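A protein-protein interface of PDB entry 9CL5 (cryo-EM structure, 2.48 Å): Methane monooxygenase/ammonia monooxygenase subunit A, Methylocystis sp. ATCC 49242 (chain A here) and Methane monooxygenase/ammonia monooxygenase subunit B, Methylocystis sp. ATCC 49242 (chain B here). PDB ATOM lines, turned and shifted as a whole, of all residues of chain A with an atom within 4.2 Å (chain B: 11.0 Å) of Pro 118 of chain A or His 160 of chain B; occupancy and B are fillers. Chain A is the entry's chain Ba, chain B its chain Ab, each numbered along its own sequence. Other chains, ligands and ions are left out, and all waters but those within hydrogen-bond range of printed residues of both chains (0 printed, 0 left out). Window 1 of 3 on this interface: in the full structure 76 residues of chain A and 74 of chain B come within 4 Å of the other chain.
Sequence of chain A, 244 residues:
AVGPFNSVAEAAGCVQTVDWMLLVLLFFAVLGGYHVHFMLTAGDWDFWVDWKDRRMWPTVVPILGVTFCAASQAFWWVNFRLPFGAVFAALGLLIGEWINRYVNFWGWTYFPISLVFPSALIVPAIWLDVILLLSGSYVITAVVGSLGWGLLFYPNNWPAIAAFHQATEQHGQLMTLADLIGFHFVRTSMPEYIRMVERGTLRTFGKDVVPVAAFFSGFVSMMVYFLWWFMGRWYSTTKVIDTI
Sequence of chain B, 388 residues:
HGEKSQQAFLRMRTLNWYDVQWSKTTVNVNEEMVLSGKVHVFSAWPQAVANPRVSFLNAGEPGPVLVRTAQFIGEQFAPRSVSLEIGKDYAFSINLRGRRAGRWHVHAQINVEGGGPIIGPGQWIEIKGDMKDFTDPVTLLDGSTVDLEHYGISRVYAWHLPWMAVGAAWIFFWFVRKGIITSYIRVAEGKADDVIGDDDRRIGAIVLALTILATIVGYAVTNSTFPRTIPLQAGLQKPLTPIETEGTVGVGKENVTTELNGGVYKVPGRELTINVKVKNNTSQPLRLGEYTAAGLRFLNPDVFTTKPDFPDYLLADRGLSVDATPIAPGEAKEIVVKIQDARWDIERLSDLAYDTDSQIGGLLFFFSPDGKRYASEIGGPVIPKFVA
The backbone carbonyl oxygen (O) of Pro 118 of chain A lies within hydrogen-bond range of a ring nitrogen (NE2) of His 160 of chain B (3.1 Å).
The side-chain carboxylate (OD1) of Asp 46 of chain A sits at hydrogen-bond distance from the side-chain hydroxyl (OG) of Ser 119 of chain A (2.6 Å). The backbone carbonyl oxygen (O) of Val 156 of chain B sits close to a ring nitrogen (ND1) of His 160 of chain B, 3.4 Å away.
CG1 of Val 156 of chain B touches CH2 of Trp 98 of chain A, at 3.7 Å. CZ3 of Trp 98 of chain A touches CE1 of Tyr 157 of chain B, at 3.6 Å. Trp 98 of chain A touches His 160 of chain B. Trp 98 of chain A touches Met 164 of chain B. Phe 117 of chain A touches Val 156 of chain B (CB to CG1, 3.8 Å). His 160 of chain B touches Ser 119 of chain A (NE2 to O, 3.6 Å). Ala 120 of chain A touches His 160 of chain B.
Of the printed residues of chain A, His 160 of chain B touches Trp 98, Pro 118, Ser 119 and Ala 120. No residue of chain B comes within 4 Å of Glu 97 of chain A. Trp 98 of chain A touches just these residues of chain B: Val 156 (3.7 Å), Tyr 157 (3.6 Å), His 160 (3.6 Å) and Met 164 (3.5 Å). Ala 120 of chain A touches just one residue of chain B: His 160. Of the printed residues of chain A, Tyr 157 of chain B touches Trp 98. Of the printed residues of chain A, Met 164 of chain B touches Trp 98. Printed residues of chain B within 4 Å of Phe 117 of chain A: Val 156 (3.8 Å). Printed residues of chain A within 4 Å of Val 156 of chain B: Trp 98 and Phe 117. The nearest residue of chain B that does not touch Pro 118 of chain A is Val 156 of chain B (6.0 Å). The nearest printed residue of chain B that does not touch Phe 117 of chain A is His 160 of chain B (4.01 Å).
Printed residues of chain A that touch a printed residue of chain B: Trp 98, Phe 117, Pro 118, Ser 119 and Ala 120. Hydrophobic or aromatic side chains of chain A that line the printed part of chain B: Trp 98, Phe 117 and Ala 120. Printed residues of chain B that touch a printed residue of chain A: Val 156, Tyr 157, His 160 and Met 164. Hydrophobic or aromatic side chains of chain B within 4 Å of the printed part of chain A: Val 156, Tyr 157, His 160 and Met 164. Among the printed residues, no Asp or Glu carboxylate lies within 4 Å of a Lys or Arg side-chain nitrogen of the other chain.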
ATOM      1  N   ASP A  46       2.142  -9.126 -18.973  1.00  0.00           N
ATOM      2  CA  ASP A  46       1.118  -8.162 -18.587  1.00  0.00           C
ATOM      3  C   ASP A  46       0.138  -7.875 -19.717  1.00  0.00           C
ATOM      4  O   ASP A  46      -1.038  -7.604 -19.455  1.00  0.00           O
ATOM      5  CB  ASP A  46       1.773  -6.861 -18.127  1.00  0.00           C
ATOM      6  CG  ASP A  46       0.995  -6.179 -17.022  1.00  0.00           C
ATOM      7  OD1 ASP A  46       0.691  -6.845 -16.014  1.00  0.00           O
ATOM      8  OD2 ASP A  46       0.687  -4.979 -17.163  1.00  0.00           O
ATOM      9  N   GLU A  97      -0.680   2.018 -17.591  1.00  0.00           N
ATOM     10  CA  GLU A  97      -1.036   0.788 -18.287  1.00  0.00           C
ATOM     11  C   GLU A  97      -2.517   0.756 -18.632  1.00  0.00           C
ATOM     12  O   GLU A  97      -2.888   0.411 -19.755  1.00  0.00           O
ATOM     13  CB  GLU A  97      -0.655  -0.422 -17.437  1.00  0.00           C
ATOM     14  CG  GLU A  97       0.771  -0.882 -17.634  1.00  0.00           C
ATOM     15  CD  GLU A  97       1.197  -1.910 -16.614  1.00  0.00           C
ATOM     16  OE1 GLU A  97       0.411  -2.193 -15.688  1.00  0.00           O
ATOM     17  OE2 GLU A  97       2.319  -2.437 -16.739  1.00  0.00           O
ATOM     18  N   TRP A  98      -3.381   1.114 -17.680  1.00  0.00           N
ATOM     19  CA  TRP A  98      -4.816   1.074 -17.938  1.00  0.00           C
ATOM     20  C   TRP A  98      -5.213   2.072 -19.015  1.00  0.00           C
ATOM     21  O   TRP A  98      -6.050   1.766 -19.876  1.00  0.00           O
ATOM     22  CB  TRP A  98      -5.594   1.335 -16.648  1.00  0.00           C
ATOM     23  CG  TRP A  98      -6.083   0.085 -15.992  1.00  0.00           C
ATOM     24  CD1 TRP A  98      -5.699  -0.410 -14.783  1.00  0.00           C
ATOM     25  CD2 TRP A  98      -7.043  -0.840 -16.519  1.00  0.00           C
ATOM     26  NE1 TRP A  98      -6.363  -1.581 -14.518  1.00  0.00           N
ATOM     27  CE2 TRP A  98      -7.194  -1.868 -15.569  1.00  0.00           C
ATOM     28  CE3 TRP A  98      -7.789  -0.897 -17.700  1.00  0.00           C
ATOM     29  CZ2 TRP A  98      -8.059  -2.940 -15.763  1.00  0.00           C
ATOM     30  CZ3 TRP A  98      -8.647  -1.962 -17.890  1.00  0.00           C
ATOM     31  CH2 TRP A  98      -8.776  -2.968 -16.927  1.00  0.00           C
ATOM     32  N   ARG A 101      -4.186   0.465 -22.331  1.00  0.00           N
ATOM     33  CA  ARG A 101      -5.027  -0.657 -22.746  1.00  0.00           C
ATOM     34  C   ARG A 101      -6.402  -0.185 -23.193  1.00  0.00           C
ATOM     35  O   ARG A 101      -6.945  -0.694 -24.180  1.00  0.00           O
ATOM     36  CB  ARG A 101      -5.169  -1.692 -21.626  1.00  0.00           C
ATOM     37  CG  ARG A 101      -3.895  -2.051 -20.905  1.00  0.00           C
ATOM     38  CD  ARG A 101      -3.025  -3.009 -21.684  1.00  0.00           C
ATOM     39  NE  ARG A 101      -1.676  -3.047 -21.132  1.00  0.00           N
ATOM     40  CZ  ARG A 101      -1.217  -4.002 -20.335  1.00  0.00           C
ATOM     41  NH1 ARG A 101      -1.967  -5.033 -19.990  1.00  0.00           N
ATOM     42  NH2 ARG A 101       0.027  -3.917 -19.874  1.00  0.00           N
ATOM     43  N   PHE A 117      -5.704  -6.712 -20.054  1.00  0.00           N
ATOM     44  CA  PHE A 117      -5.827  -5.967 -18.815  1.00  0.00           C
ATOM     45  C   PHE A 117      -4.555  -6.199 -18.014  1.00  0.00           C
ATOM     46  O   PHE A 117      -3.983  -7.298 -18.062  1.00  0.00           O
ATOM     47  CB  PHE A 117      -7.069  -6.367 -17.998  1.00  0.00           C
ATOM     48  CG  PHE A 117      -7.120  -7.819 -17.611  1.00  0.00           C
ATOM     49  CD1 PHE A 117      -6.563  -8.256 -16.419  1.00  0.00           C
ATOM     50  CD2 PHE A 117      -7.752  -8.745 -18.426  1.00  0.00           C
ATOM     51  CE1 PHE A 117      -6.620  -9.587 -16.058  1.00  0.00           C
ATOM     52  CE2 PHE A 117      -7.810 -10.075 -18.069  1.00  0.00           C
ATOM     53  CZ  PHE A 117      -7.244 -10.496 -16.884  1.00  0.00           C
ATOM     54  N   PRO A 118      -4.081  -5.193 -17.287  1.00  0.00           N
ATOM     55  CA  PRO A 118      -2.799  -5.317 -16.590  1.00  0.00           C
ATOM     56  C   PRO A 118      -2.937  -6.106 -15.295  1.00  0.00           C
ATOM     57  O   PRO A 118      -4.031  -6.449 -14.847  1.00  0.00           O
ATOM     58  CB  PRO A 118      -2.387  -3.866 -16.313  1.00  0.00           C
ATOM     59  CG  PRO A 118      -3.603  -3.035 -16.537  1.00  0.00           C
ATOM     60  CD  PRO A 118      -4.706  -3.874 -17.092  1.00  0.00           C
ATOM     61  N   SER A 119      -1.784  -6.408 -14.703  1.00  0.00           N
ATOM     62  CA  SER A 119      -1.750  -7.083 -13.416  1.00  0.00           C
ATOM     63  C   SER A 119      -2.057  -6.100 -12.290  1.00  0.00           C
ATOM     64  O   SER A 119      -2.034  -4.880 -12.467  1.00  0.00           O
ATOM     65  CB  SER A 119      -0.385  -7.731 -13.189  1.00  0.00           C
ATOM     66  OG  SER A 119      -0.057  -8.606 -14.251  1.00  0.00           O
ATOM     67  N   ALA A 120      -2.345  -6.651 -11.116  1.00  0.00           N
ATOM     68  CA  ALA A 120      -2.650  -5.858  -9.933  1.00  0.00           C
ATOM     69  C   ALA A 120      -1.437  -5.831  -9.012  1.00  0.00           C
ATOM     70  O   ALA A 120      -0.897  -6.883  -8.657  1.00  0.00           O
ATOM     71  CB  ALA A 120      -3.867  -6.421  -9.197  1.00  0.00           C
ATOM     72  N   GLY B 152     -16.534 -11.306 -18.487  1.00  0.00           N
ATOM     73  CA  GLY B 152     -15.462 -11.162 -17.527  1.00  0.00           C
ATOM     74  C   GLY B 152     -14.859  -9.781 -17.399  1.00  0.00           C
ATOM     75  O   GLY B 152     -13.961  -9.594 -16.571  1.00  0.00           O
ATOM     76  N   ILE B 153     -15.322  -8.804 -18.181  1.00  0.00           N
ATOM     77  CA  ILE B 153     -14.717  -7.477 -18.148  1.00  0.00           C
ATOM     78  C   ILE B 153     -15.202  -6.688 -16.935  1.00  0.00           C
ATOM     79  O   ILE B 153     -14.438  -5.923 -16.328  1.00  0.00           O
ATOM     80  CB  ILE B 153     -15.007  -6.744 -19.470  1.00  0.00           C
ATOM     81  CG1 ILE B 153     -14.402  -7.516 -20.645  1.00  0.00           C
ATOM     82  CG2 ILE B 153     -14.443  -5.344 -19.446  1.00  0.00           C
ATOM     83  CD1 ILE B 153     -14.723  -6.922 -21.995  1.00  0.00           C
ATOM     84  N   SER B 154     -16.468  -6.874 -16.557  1.00  0.00           N
ATOM     85  CA  SER B 154     -17.011  -6.183 -15.391  1.00  0.00           C
ATOM     86  C   SER B 154     -16.278  -6.585 -14.120  1.00  0.00           C
ATOM     87  O   SER B 154     -16.009  -5.741 -13.259  1.00  0.00           O
ATOM     88  CB  SER B 154     -18.505  -6.469 -15.260  1.00  0.00           C
ATOM     89  OG  SER B 154     -19.265  -5.575 -16.052  1.00  0.00           O
ATOM     90  N   ARG B 155     -15.954  -7.873 -13.979  1.00  0.00           N
ATOM     91  CA  ARG B 155     -15.176  -8.323 -12.829  1.00  0.00           C
ATOM     92  C   ARG B 155     -13.796  -7.679 -12.818  1.00  0.00           C
ATOM     93  O   ARG B 155     -13.295  -7.280 -11.758  1.00  0.00           O
ATOM     94  CB  ARG B 155     -15.054  -9.845 -12.847  1.00  0.00           C
ATOM     95  CG  ARG B 155     -16.322 -10.565 -12.437  1.00  0.00           C
ATOM     96  CD  ARG B 155     -16.022 -11.903 -11.787  1.00  0.00           C
ATOM     97  NE  ARG B 155     -17.250 -12.565 -11.362  1.00  0.00           N
ATOM     98  CZ  ARG B 155     -17.627 -12.701 -10.100  1.00  0.00           C
ATOM     99  NH1 ARG B 155     -16.876 -12.266  -9.103  1.00  0.00           N
ATOM    100  NH2 ARG B 155     -18.789 -13.289  -9.830  1.00  0.00           N
ATOM    101  N   VAL B 156     -13.168  -7.568 -13.991  1.00  0.00           N
ATOM    102  CA  VAL B 156     -11.849  -6.951 -14.080  1.00  0.00           C
ATOM    103  C   VAL B 156     -11.907  -5.506 -13.605  1.00  0.00           C
ATOM    104  O   VAL B 156     -11.074  -5.064 -12.806  1.00  0.00           O
ATOM    105  CB  VAL B 156     -11.303  -7.056 -15.516  1.00  0.00           C
ATOM    106  CG1 VAL B 156     -10.075  -6.175 -15.683  1.00  0.00           C
ATOM    107  CG2 VAL B 156     -10.976  -8.499 -15.856  1.00  0.00           C
ATOM    108  N   TYR B 157     -12.900  -4.750 -14.081  1.00  0.00           N
ATOM    109  CA  TYR B 157     -13.035  -3.365 -13.633  1.00  0.00           C
ATOM    110  C   TYR B 157     -13.317  -3.291 -12.136  1.00  0.00           C
ATOM    111  O   TYR B 157     -12.679  -2.521 -11.410  1.00  0.00           O
ATOM    112  CB  TYR B 157     -14.135  -2.646 -14.413  1.00  0.00           C
ATOM    113  CG  TYR B 157     -13.800  -2.353 -15.854  1.00  0.00           C
ATOM    114  CD1 TYR B 157     -12.545  -1.882 -16.210  1.00  0.00           C
ATOM    115  CD2 TYR B 157     -14.754  -2.491 -16.850  1.00  0.00           C
ATOM    116  CE1 TYR B 157     -12.236  -1.597 -17.523  1.00  0.00           C
ATOM    117  CE2 TYR B 157     -14.456  -2.201 -18.163  1.00  0.00           C
ATOM    118  CZ  TYR B 157     -13.198  -1.758 -18.495  1.00  0.00           C
ATOM    119  OH  TYR B 157     -12.897  -1.471 -19.806  1.00  0.00           O
ATOM    120  N   ALA B 158     -14.269  -4.097 -11.656  1.00  0.00           N
ATOM    121  CA  ALA B 158     -14.672  -4.041 -10.257  1.00  0.00           C
ATOM    122  C   ALA B 158     -13.555  -4.444  -9.311  1.00  0.00           C
ATOM    123  O   ALA B 158     -13.588  -4.061  -8.138  1.00  0.00           O
ATOM    124  CB  ALA B 158     -15.893  -4.933 -10.029  1.00  0.00           C
ATOM    125  N   TRP B 159     -12.577  -5.216  -9.780  1.00  0.00           N
ATOM    126  CA  TRP B 159     -11.428  -5.506  -8.933  1.00  0.00           C
ATOM    127  C   TRP B 159     -10.316  -4.475  -9.085  1.00  0.00           C
ATOM    128  O   TRP B 159      -9.651  -4.137  -8.102  1.00  0.00           O
ATOM    129  CB  TRP B 159     -10.885  -6.906  -9.227  1.00  0.00           C
ATOM    130  CG  TRP B 159      -9.767  -7.300  -8.310  1.00  0.00           C
ATOM    131  CD1 TRP B 159      -8.456  -7.461  -8.642  1.00  0.00           C
ATOM    132  CD2 TRP B 159      -9.862  -7.562  -6.905  1.00  0.00           C
ATOM    133  NE1 TRP B 159      -7.728  -7.816  -7.534  1.00  0.00           N
ATOM    134  CE2 TRP B 159      -8.568  -7.885  -6.453  1.00  0.00           C
ATOM    135  CE3 TRP B 159     -10.916  -7.561  -5.988  1.00  0.00           C
ATOM    136  CZ2 TRP B 159      -8.299  -8.203  -5.124  1.00  0.00           C
ATOM    137  CZ3 TRP B 159     -10.647  -7.878  -4.668  1.00  0.00           C
ATOM    138  CH2 TRP B 159      -9.350  -8.194  -4.250  1.00  0.00           C
ATOM    139  N   HIS B 160     -10.104  -3.947 -10.293  1.00  0.00           N
ATOM    140  CA  HIS B 160      -8.931  -3.116 -10.535  1.00  0.00           C
ATOM    141  C   HIS B 160      -9.157  -1.664 -10.129  1.00  0.00           C
ATOM    142  O   HIS B 160      -8.300  -1.059  -9.474  1.00  0.00           O
ATOM    143  CB  HIS B 160      -8.532  -3.208 -12.007  1.00  0.00           C
ATOM    144  CG  HIS B 160      -7.450  -4.205 -12.275  1.00  0.00           C
ATOM    145  ND1 HIS B 160      -7.660  -5.353 -13.008  1.00  0.00           N
ATOM    146  CD2 HIS B 160      -6.145  -4.223 -11.917  1.00  0.00           C
ATOM    147  CE1 HIS B 160      -6.533  -6.038 -13.083  1.00  0.00           C
ATOM    148  NE2 HIS B 160      -5.597  -5.372 -12.431  1.00  0.00           N
ATOM    149  N   LEU B 161     -10.288  -1.078 -10.521  1.00  0.00           N
ATOM    150  CA  LEU B 161     -10.499   0.349 -10.277  1.00  0.00           C
ATOM    151  C   LEU B 161     -10.565   0.710  -8.796  1.00  0.00           C
ATOM    152  O   LEU B 161      -9.946   1.717  -8.405  1.00  0.00           O
ATOM    153  CB  LEU B 161     -11.751   0.816 -11.030  1.00  0.00           C
ATOM    154  CG  LEU B 161     -11.737   0.597 -12.546  1.00  0.00           C
ATOM    155  CD1 LEU B 161     -12.958   1.228 -13.189  1.00  0.00           C
ATOM    156  CD2 LEU B 161     -10.458   1.132 -13.167  1.00  0.00           C
ATOM    157  N   PRO B 162     -11.296  -0.014  -7.935  1.00  0.00           N
ATOM    158  CA  PRO B 162     -11.307   0.365  -6.510  1.00  0.00           C
ATOM    159  C   PRO B 162      -9.936   0.358  -5.856  1.00  0.00           C
ATOM    160  O   PRO B 162      -9.671   1.199  -4.990  1.00  0.00           O
ATOM    161  CB  PRO B 162     -12.242  -0.675  -5.881  1.00  0.00           C
ATOM    162  CG  PRO B 162     -13.134  -1.085  -6.979  1.00  0.00           C
ATOM    163  CD  PRO B 162     -12.305  -1.052  -8.222  1.00  0.00           C
ATOM    164  N   TRP B 163      -9.051  -0.565  -6.236  1.00  0.00           N
ATOM    165  CA  TRP B 163      -7.719  -0.583  -5.636  1.00  0.00           C
ATOM    166  C   TRP B 163      -6.892   0.617  -6.084  1.00  0.00           C
ATOM    167  O   TRP B 163      -6.117   1.176  -5.297  1.00  0.00           O
ATOM    168  CB  TRP B 163      -7.010  -1.893  -5.970  1.00  0.00           C
ATOM    169  CG  TRP B 163      -7.477  -3.037  -5.125  1.00  0.00           C
ATOM    170  CD1 TRP B 163      -8.136  -4.150  -5.548  1.00  0.00           C
ATOM    171  CD2 TRP B 163      -7.335  -3.172  -3.706  1.00  0.00           C
ATOM    172  NE1 TRP B 163      -8.409  -4.972  -4.485  1.00  0.00           N
ATOM    173  CE2 TRP B 163      -7.926  -4.395  -3.341  1.00  0.00           C
ATOM    174  CE3 TRP B 163      -6.760  -2.377  -2.708  1.00  0.00           C
ATOM    175  CZ2 TRP B 163      -7.961  -4.845  -2.023  1.00  0.00           C
ATOM    176  CZ3 TRP B 163      -6.795  -2.825  -1.402  1.00  0.00           C
ATOM    177  CH2 TRP B 163      -7.392  -4.048  -1.070  1.00  0.00           C
ATOM    178  N   MET B 164      -7.045   1.031  -7.344  1.00  0.00           N
ATOM    179  CA  MET B 164      -6.398   2.256  -7.800  1.00  0.00           C
ATOM    180  C   MET B 164      -6.925   3.466  -7.043  1.00  0.00           C
ATOM    181  O   MET B 164      -6.157   4.367  -6.681  1.00  0.00           O
ATOM    182  CB  MET B 164      -6.609   2.425  -9.304  1.00  0.00           C
ATOM    183  CG  MET B 164      -5.857   1.418 -10.153  1.00  0.00           C
ATOM    184  SD  MET B 164      -6.480   1.348 -11.840  1.00  0.00           S
ATOM    185  CE  MET B 164      -5.355   2.471 -12.654  1.00  0.00           C
ATOM    186  N   ALA B 165      -8.236   3.501  -6.792  1.00  0.00           N
ATOM    187  CA  ALA B 165      -8.803   4.583  -5.993  1.00  0.00           C
ATOM    188  C   ALA B 165      -8.237   4.575  -4.578  1.00  0.00           C
ATOM    189  O   ALA B 165      -7.947   5.634  -4.011  1.00  0.00           O
ATOM    190  CB  ALA B 165     -10.326   4.473  -5.965  1.00  0.00           C
ATOM    191  N   VAL B 166      -8.076   3.386  -3.992  1.00  0.00           N
ATOM    192  CA  VAL B 166      -7.515   3.274  -2.648  1.00  0.00           C
ATOM    193  C   VAL B 166      -6.077   3.783  -2.618  1.00  0.00           C
ATOM    194  O   VAL B 166      -5.676   4.500  -1.693  1.00  0.00           O
ATOM    195  CB  VAL B 166      -7.613   1.818  -2.151  1.00  0.00           C
ATOM    196  CG1 VAL B 166      -6.714   1.596  -0.946  1.00  0.00           C
ATOM    197  CG2 VAL B 166      -9.050   1.471  -1.813  1.00  0.00           C
ATOM    198  N   GLY B 167      -5.276   3.415  -3.619  1.00  0.00           N
ATOM    199  CA  GLY B 167      -3.905   3.902  -3.673  1.00  0.00           C
ATOM    200  C   GLY B 167      -3.823   5.409  -3.835  1.00  0.00           C
ATOM    201  O   GLY B 167      -3.007   6.075  -3.185  1.00  0.00           O
ATOM    202  N   ALA B 168      -4.671   5.967  -4.702  1.00  0.00           N
ATOM    203  CA  ALA B 168      -4.719   7.414  -4.860  1.00  0.00           C
ATOM    204  C   ALA B 168      -5.125   8.093  -3.559  1.00  0.00           C
ATOM    205  O   ALA B 168      -4.573   9.137  -3.196  1.00  0.00           O
ATOM    206  CB  ALA B 168      -5.679   7.792  -5.986  1.00  0.00           C
ATOM    207  N   THR B 222     -13.977 -15.277  -4.695  1.00  0.00           N
ATOM    208  CA  THR B 222     -13.675 -15.708  -6.054  1.00  0.00           C
ATOM    209  C   THR B 222     -13.639 -17.225  -6.158  1.00  0.00           C
ATOM    210  O   THR B 222     -14.154 -17.801  -7.123  1.00  0.00           O
ATOM    211  CB  THR B 222     -12.346 -15.101  -6.503  1.00  0.00           C
ATOM    212  OG1 THR B 222     -12.403 -13.679  -6.364  1.00  0.00           O
ATOM    213  CG2 THR B 222     -12.078 -15.438  -7.944  1.00  0.00           C
